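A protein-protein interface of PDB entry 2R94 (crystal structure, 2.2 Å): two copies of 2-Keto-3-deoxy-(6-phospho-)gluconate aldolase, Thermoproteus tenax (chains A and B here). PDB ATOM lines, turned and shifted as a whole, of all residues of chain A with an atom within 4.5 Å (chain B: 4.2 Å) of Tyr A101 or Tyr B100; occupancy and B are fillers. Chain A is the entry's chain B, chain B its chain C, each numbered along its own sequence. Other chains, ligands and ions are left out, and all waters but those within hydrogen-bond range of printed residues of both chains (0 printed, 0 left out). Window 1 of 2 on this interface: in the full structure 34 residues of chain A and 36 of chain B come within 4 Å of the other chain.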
ATOM      1  N   LEU A  74     -16.919  11.249 -21.882  1.00  0.00           N
ATOM      2  CA  LEU A  74     -16.928  12.570 -22.518  1.00  0.00           C
ATOM      3  C   LEU A  74     -16.219  12.543 -23.878  1.00  0.00           C
ATOM      4  O   LEU A  74     -16.033  13.579 -24.502  1.00  0.00           O
ATOM      5  CB  LEU A  74     -16.291  13.591 -21.587  1.00  0.00           C
ATOM      6  CG  LEU A  74     -17.121  13.820 -20.295  1.00  0.00           C
ATOM      7  CD1 LEU A  74     -16.431  14.842 -19.381  1.00  0.00           C
ATOM      8  CD2 LEU A  74     -18.579  14.285 -20.620  1.00  0.00           C
ATOM      9  N   TYR A 100     -22.119  14.765 -19.036  1.00  0.00           N
ATOM     10  CA  TYR A 100     -21.869  15.479 -17.798  1.00  0.00           C
ATOM     11  C   TYR A 100     -20.738  16.503 -17.905  1.00  0.00           C
ATOM     12  O   TYR A 100     -20.156  16.712 -18.978  1.00  0.00           O
ATOM     13  CB  TYR A 100     -21.517  14.485 -16.700  1.00  0.00           C
ATOM     14  CG  TYR A 100     -20.443  13.461 -17.050  1.00  0.00           C
ATOM     15  CD1 TYR A 100     -19.141  13.600 -16.575  1.00  0.00           C
ATOM     16  CD2 TYR A 100     -20.735  12.360 -17.848  1.00  0.00           C
ATOM     17  CE1 TYR A 100     -18.168  12.724 -16.898  1.00  0.00           C
ATOM     18  CE2 TYR A 100     -19.771  11.432 -18.148  1.00  0.00           C
ATOM     19  CZ  TYR A 100     -18.484  11.624 -17.649  1.00  0.00           C
ATOM     20  OH  TYR A 100     -17.513  10.701 -17.940  1.00  0.00           O
ATOM     21  N   TYR A 101     -20.469  17.177 -16.782  1.00  0.00           N
ATOM     22  CA  TYR A 101     -19.424  18.222 -16.680  1.00  0.00           C
ATOM     23  C   TYR A 101     -19.762  19.530 -17.373  1.00  0.00           C
ATOM     24  O   TYR A 101     -19.895  20.593 -16.721  1.00  0.00           O
ATOM     25  CB  TYR A 101     -18.020  17.778 -17.112  1.00  0.00           C
ATOM     26  CG  TYR A 101     -17.099  18.984 -16.879  1.00  0.00           C
ATOM     27  CD1 TYR A 101     -16.684  19.299 -15.604  1.00  0.00           C
ATOM     28  CD2 TYR A 101     -16.758  19.851 -17.925  1.00  0.00           C
ATOM     29  CE1 TYR A 101     -15.925  20.406 -15.343  1.00  0.00           C
ATOM     30  CE2 TYR A 101     -15.979  20.958 -17.682  1.00  0.00           C
ATOM     31  CZ  TYR A 101     -15.588  21.248 -16.373  1.00  0.00           C
ATOM     32  OH  TYR A 101     -14.859  22.371 -16.119  1.00  0.00           O
ATOM     33  N   PHE A 102     -19.846  19.477 -18.697  1.00  0.00           N
ATOM     34  CA  PHE A 102     -19.946  20.683 -19.509  1.00  0.00           C
ATOM     35  C   PHE A 102     -21.303  21.296 -19.283  1.00  0.00           C
ATOM     36  O   PHE A 102     -22.335  20.673 -19.572  1.00  0.00           O
ATOM     37  CB  PHE A 102     -19.799  20.326 -20.991  1.00  0.00           C
ATOM     38  CG  PHE A 102     -18.418  19.874 -21.354  1.00  0.00           C
ATOM     39  CD1 PHE A 102     -17.371  20.771 -21.381  1.00  0.00           C
ATOM     40  CD2 PHE A 102     -18.151  18.538 -21.580  1.00  0.00           C
ATOM     41  CE1 PHE A 102     -16.091  20.369 -21.685  1.00  0.00           C
ATOM     42  CE2 PHE A 102     -16.854  18.107 -21.897  1.00  0.00           C
ATOM     43  CZ  PHE A 102     -15.829  19.019 -21.947  1.00  0.00           C
ATOM     44  N   PRO A 103     -21.335  22.517 -18.757  1.00  0.00           N
ATOM     45  CA  PRO A 103     -22.675  23.052 -18.540  1.00  0.00           C
ATOM     46  C   PRO A 103     -23.368  23.486 -19.851  1.00  0.00           C
ATOM     47  O   PRO A 103     -24.601  23.575 -19.935  1.00  0.00           O
ATOM     48  CB  PRO A 103     -22.433  24.272 -17.634  1.00  0.00           C
ATOM     49  CG  PRO A 103     -20.963  24.272 -17.296  1.00  0.00           C
ATOM     50  CD  PRO A 103     -20.271  23.451 -18.346  1.00  0.00           C
ATOM     51  N   VAL A 134     -24.330  14.836 -12.449  1.00  0.00           N
ATOM     52  CA  VAL A 134     -24.183  15.065 -13.849  1.00  0.00           C
ATOM     53  C   VAL A 134     -24.299  16.536 -14.190  1.00  0.00           C
ATOM     54  O   VAL A 134     -23.695  16.992 -15.161  1.00  0.00           O
ATOM     55  CB  VAL A 134     -25.259  14.286 -14.610  1.00  0.00           C
ATOM     56  CG1 VAL A 134     -25.448  14.854 -16.024  1.00  0.00           C
ATOM     57  CG2 VAL A 134     -24.872  12.853 -14.617  1.00  0.00           C
ATOM     58  N   THR B  41     -12.169  24.384 -20.001  1.00  0.00           N
ATOM     59  CA  THR B  41     -13.514  23.894 -20.259  1.00  0.00           C
ATOM     60  C   THR B  41     -13.842  24.257 -21.675  1.00  0.00           C
ATOM     61  O   THR B  41     -14.341  23.407 -22.407  1.00  0.00           O
ATOM     62  CB  THR B  41     -14.596  24.580 -19.300  1.00  0.00           C
ATOM     63  OG1 THR B  41     -14.384  24.139 -17.953  1.00  0.00           O
ATOM     64  CG2 THR B  41     -16.013  24.208 -19.700  1.00  0.00           C
ATOM     65  N   PRO B  46     -11.770  18.164 -19.993  1.00  0.00           N
ATOM     66  CA  PRO B  46     -12.332  16.935 -19.481  1.00  0.00           C
ATOM     67  C   PRO B  46     -12.729  15.872 -20.537  1.00  0.00           C
ATOM     68  O   PRO B  46     -12.874  14.713 -20.190  1.00  0.00           O
ATOM     69  CB  PRO B  46     -13.567  17.454 -18.710  1.00  0.00           C
ATOM     70  CG  PRO B  46     -13.003  18.786 -18.136  1.00  0.00           C
ATOM     71  CD  PRO B  46     -12.415  19.354 -19.376  1.00  0.00           C
ATOM     72  N   ALA B  72      -6.572  18.921 -15.045  1.00  0.00           N
ATOM     73  CA  ALA B  72      -7.441  18.055 -14.247  1.00  0.00           C
ATOM     74  C   ALA B  72      -7.714  16.752 -14.940  1.00  0.00           C
ATOM     75  O   ALA B  72      -7.888  16.666 -16.151  1.00  0.00           O
ATOM     76  CB  ALA B  72      -8.709  18.733 -13.915  1.00  0.00           C
ATOM     77  N   LEU B  74      -9.860  12.849 -13.807  1.00  0.00           N
ATOM     78  CA  LEU B  74     -10.456  12.018 -12.768  1.00  0.00           C
ATOM     79  C   LEU B  74      -9.575  10.794 -12.421  1.00  0.00           C
ATOM     80  O   LEU B  74      -9.983   9.927 -11.635  1.00  0.00           O
ATOM     81  CB  LEU B  74     -11.890  11.620 -13.130  1.00  0.00           C
ATOM     82  CG  LEU B  74     -12.869  12.791 -13.158  1.00  0.00           C
ATOM     83  CD1 LEU B  74     -14.264  12.315 -13.461  1.00  0.00           C
ATOM     84  CD2 LEU B  74     -12.826  13.476 -11.836  1.00  0.00           C
ATOM     85  N   LEU B  97      -8.888  22.319 -12.405  1.00  0.00           N
ATOM     86  CA  LEU B  97     -10.187  22.137 -11.768  1.00  0.00           C
ATOM     87  C   LEU B  97      -9.986  21.274 -10.513  1.00  0.00           C
ATOM     88  O   LEU B  97      -9.043  20.466 -10.447  1.00  0.00           O
ATOM     89  CB  LEU B  97     -11.129  21.344 -12.705  1.00  0.00           C
ATOM     90  CG  LEU B  97     -11.574  22.040 -13.975  1.00  0.00           C
ATOM     91  CD1 LEU B  97     -12.113  20.999 -15.022  1.00  0.00           C
ATOM     92  CD2 LEU B  97     -12.606  23.134 -13.662  1.00  0.00           C
ATOM     93  N   PRO B  98     -10.881  21.397  -9.526  1.00  0.00           N
ATOM     94  CA  PRO B  98     -10.853  20.443  -8.457  1.00  0.00           C
ATOM     95  C   PRO B  98     -11.441  19.145  -8.961  1.00  0.00           C
ATOM     96  O   PRO B  98     -12.187  19.142  -9.960  1.00  0.00           O
ATOM     97  CB  PRO B  98     -11.847  21.041  -7.428  1.00  0.00           C
ATOM     98  CG  PRO B  98     -11.972  22.478  -7.809  1.00  0.00           C
ATOM     99  CD  PRO B  98     -11.886  22.453  -9.306  1.00  0.00           C
ATOM    100  N   PRO B  99     -11.220  18.041  -8.222  1.00  0.00           N
ATOM    101  CA  PRO B  99     -11.893  16.824  -8.609  1.00  0.00           C
ATOM    102  C   PRO B  99     -13.400  17.084  -8.828  1.00  0.00           C
ATOM    103  O   PRO B  99     -14.080  17.691  -7.973  1.00  0.00           O
ATOM    104  CB  PRO B  99     -11.645  15.911  -7.406  1.00  0.00           C
ATOM    105  CG  PRO B  99     -10.290  16.392  -6.851  1.00  0.00           C
ATOM    106  CD  PRO B  99     -10.347  17.878  -7.038  1.00  0.00           C
ATOM    107  N   TYR B 100     -13.923  16.606  -9.944  1.00  0.00           N
ATOM    108  CA  TYR B 100     -15.265  16.951 -10.351  1.00  0.00           C
ATOM    109  C   TYR B 100     -16.082  15.714 -10.550  1.00  0.00           C
ATOM    110  O   TYR B 100     -15.603  14.624 -10.265  1.00  0.00           O
ATOM    111  CB  TYR B 100     -15.255  17.763 -11.632  1.00  0.00           C
ATOM    112  CG  TYR B 100     -14.431  17.185 -12.758  1.00  0.00           C
ATOM    113  CD1 TYR B 100     -15.027  16.369 -13.743  1.00  0.00           C
ATOM    114  CD2 TYR B 100     -13.029  17.448 -12.845  1.00  0.00           C
ATOM    115  CE1 TYR B 100     -14.270  15.833 -14.774  1.00  0.00           C
ATOM    116  CE2 TYR B 100     -12.266  16.900 -13.870  1.00  0.00           C
ATOM    117  CZ  TYR B 100     -12.902  16.112 -14.832  1.00  0.00           C
ATOM    118  OH  TYR B 100     -12.172  15.586 -15.840  1.00  0.00           O
ATOM    119  N   TYR B 101     -17.329  15.880 -11.011  1.00  0.00           N
ATOM    120  CA  TYR B 101     -18.312  14.770 -11.119  1.00  0.00           C
ATOM    121  C   TYR B 101     -18.730  14.145  -9.758  1.00  0.00           C
ATOM    122  O   TYR B 101     -19.905  14.173  -9.385  1.00  0.00           O
ATOM    123  CB  TYR B 101     -17.925  13.666 -12.166  1.00  0.00           C
ATOM    124  CG  TYR B 101     -19.036  12.627 -12.262  1.00  0.00           C
ATOM    125  CD1 TYR B 101     -20.113  12.805 -13.093  1.00  0.00           C
ATOM    126  CD2 TYR B 101     -19.051  11.540 -11.402  1.00  0.00           C
ATOM    127  CE1 TYR B 101     -21.169  11.904 -13.108  1.00  0.00           C
ATOM    128  CE2 TYR B 101     -20.094  10.667 -11.370  1.00  0.00           C
ATOM    129  CZ  TYR B 101     -21.163  10.862 -12.209  1.00  0.00           C
ATOM    130  OH  TYR B 101     -22.194   9.966 -12.147  1.00  0.00           O
ATOM    131  N   PHE B 102     -17.799  13.568  -9.023  1.00  0.00           N
ATOM    132  CA  PHE B 102     -18.188  12.752  -7.888  1.00  0.00           C
ATOM    133  C   PHE B 102     -18.689  13.666  -6.807  1.00  0.00           C
ATOM    134  O   PHE B 102     -18.003  14.593  -6.434  1.00  0.00           O
ATOM    135  CB  PHE B 102     -17.002  11.879  -7.419  1.00  0.00           C
ATOM    136  CG  PHE B 102     -16.594  10.817  -8.432  1.00  0.00           C
ATOM    137  CD1 PHE B 102     -17.367   9.664  -8.604  1.00  0.00           C
ATOM    138  CD2 PHE B 102     -15.467  10.982  -9.232  1.00  0.00           C
ATOM    139  CE1 PHE B 102     -17.004   8.692  -9.548  1.00  0.00           C
ATOM    140  CE2 PHE B 102     -15.093  10.022 -10.143  1.00  0.00           C
ATOM    141  CZ  PHE B 102     -15.873   8.875 -10.318  1.00  0.00           C
ATOM    142  N   TYR B 130     -14.685  26.317 -10.724  1.00  0.00           N
ATOM    143  CA  TYR B 130     -15.800  26.465 -11.641  1.00  0.00           C
ATOM    144  C   TYR B 130     -16.959  25.719 -11.023  1.00  0.00           C
ATOM    145  O   TYR B 130     -17.357  24.662 -11.505  1.00  0.00           O
ATOM    146  CB  TYR B 130     -15.436  25.888 -12.994  1.00  0.00           C
ATOM    147  CG  TYR B 130     -16.436  26.150 -14.097  1.00  0.00           C
ATOM    148  CD1 TYR B 130     -16.139  25.813 -15.413  1.00  0.00           C
ATOM    149  CD2 TYR B 130     -17.668  26.747 -13.838  1.00  0.00           C
ATOM    150  CE1 TYR B 130     -17.030  26.006 -16.418  1.00  0.00           C
ATOM    151  CE2 TYR B 130     -18.553  26.980 -14.836  1.00  0.00           C
ATOM    152  CZ  TYR B 130     -18.230  26.599 -16.126  1.00  0.00           C
ATOM    153  OH  TYR B 130     -19.102  26.822 -17.167  1.00  0.00           O
ATOM    154  N   ALA B 133     -19.842  23.823 -13.057  1.00  0.00           N
ATOM    155  CA  ALA B 133     -19.423  22.629 -13.804  1.00  0.00           C
ATOM    156  C   ALA B 133     -18.888  21.566 -12.895  1.00  0.00           C
ATOM    157  O   ALA B 133     -19.096  20.389 -13.123  1.00  0.00           O
ATOM    158  CB  ALA B 133     -18.338  22.981 -14.832  1.00  0.00           C
ATOM    159  N   VAL B 134     -18.131  21.978 -11.877  1.00  0.00           N
ATOM    160  CA  VAL B 134     -17.396  21.013 -11.056  1.00  0.00           C
ATOM    161  C   VAL B 134     -18.282  20.402  -9.999  1.00  0.00           C
ATOM    162  O   VAL B 134     -18.088  19.245  -9.603  1.00  0.00           O
ATOM    163  CB  VAL B 134     -16.154  21.712 -10.392  1.00  0.00           C
ATOM    164  CG1 VAL B 134     -15.574  20.872  -9.275  1.00  0.00           C
ATOM    165  CG2 VAL B 134     -15.086  22.061 -11.471  1.00  0.00           C
ATOM    166  N   ARG B 136     -18.607  21.656  -6.955  1.00  0.00           N
ATOM    167  CA  ARG B 136     -18.104  22.022  -5.642  1.00  0.00           C
ATOM    168  C   ARG B 136     -17.291  23.276  -5.877  1.00  0.00           C
ATOM    169  O   ARG B 136     -16.914  23.569  -7.008  1.00  0.00           O
ATOM    170  CB  ARG B 136     -17.243  20.931  -4.984  1.00  0.00           C
ATOM    171  CG  ARG B 136     -16.041  20.477  -5.831  1.00  0.00           C
ATOM    172  CD  ARG B 136     -15.141  19.443  -5.109  1.00  0.00           C
ATOM    173  NE  ARG B 136     -15.953  18.391  -4.473  1.00  0.00           N
ATOM    174  CZ  ARG B 136     -16.541  17.354  -5.084  1.00  0.00           C
ATOM    175  NH1 ARG B 136     -16.380  17.088  -6.386  1.00  0.00           N
ATOM    176  NH2 ARG B 136     -17.269  16.544  -4.343  1.00  0.00           N
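OG1 of Thr B41 is in hydrogen-bond range of OH of Tyr A101 (2.6 Å).
Leu A74 touches Pro B46. Tyr A100 touches Tyr B101 (CD1 to CD1, 3.7 Å). CE2 of Tyr A101 touches CG of Pro B46, 3.7 Å away. Tyr A101 touches Leu B97 (OH to CD1, 3.3 Å). CD1 of Tyr A101 touches CD1 of Tyr B100, 3.8 Å away. Tyr A101 touches Tyr B130 (OH to CD1, 3.7 Å). Tyr A101 touches Ala B133 (O to CB, 3.4 Å). CE1 of Phe A102 touches O of Thr B41, at 3.6 Å. Pro A103 touches Tyr B130 (CG to OH, 3.2 Å). CG of Pro A103 touches CB of Ala B133, 3.8 Å away.
Tyr A101 touches six residues of chain B. Of chain A, only Tyr A101 (3.8 Å) comes within 4 Å of Tyr B100. Printed residues of chain A within 4 Å of Ala B133: Tyr A101 (3.4 Å) and Pro A103 (3.8 Å). Of the printed residues of chain B, Phe A102 touches Thr B41 (3.6 Å). Of the printed residues of chain A, Tyr B101 touches Tyr A100. Printed residues of chain B within 4 Å of Pro A103: Tyr B130 and Ala B133. The nearest printed residue of chain A that does not touch Tyr B100 is Leu A74 (5.2 Å). The nearest printed residue of chain A that does not touch Ala B133 is Phe A102 (5.4 Å).
Hydrophobic or aromatic side chains of chain B within 4 Å of the printed part of chain A: Pro B46, Leu B97, Tyr B100, Tyr B101, Tyr B130 and Ala B133. Along chain B the printed residues that touch a printed residue of chain A span positions 41 to 133. Among the printed residues, no Asp or Glu carboxylate lies within 4 Å of a Lys or Arg side-chain nitrogen of the other chain.
Tyr A100 touches Tyr B101, and with the chains exchanged Tyr A101 touches Tyr B100. Of the 11 pairs that touch across the chains among the printed residues, 2 have their exchanged pair printed and touching as well.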
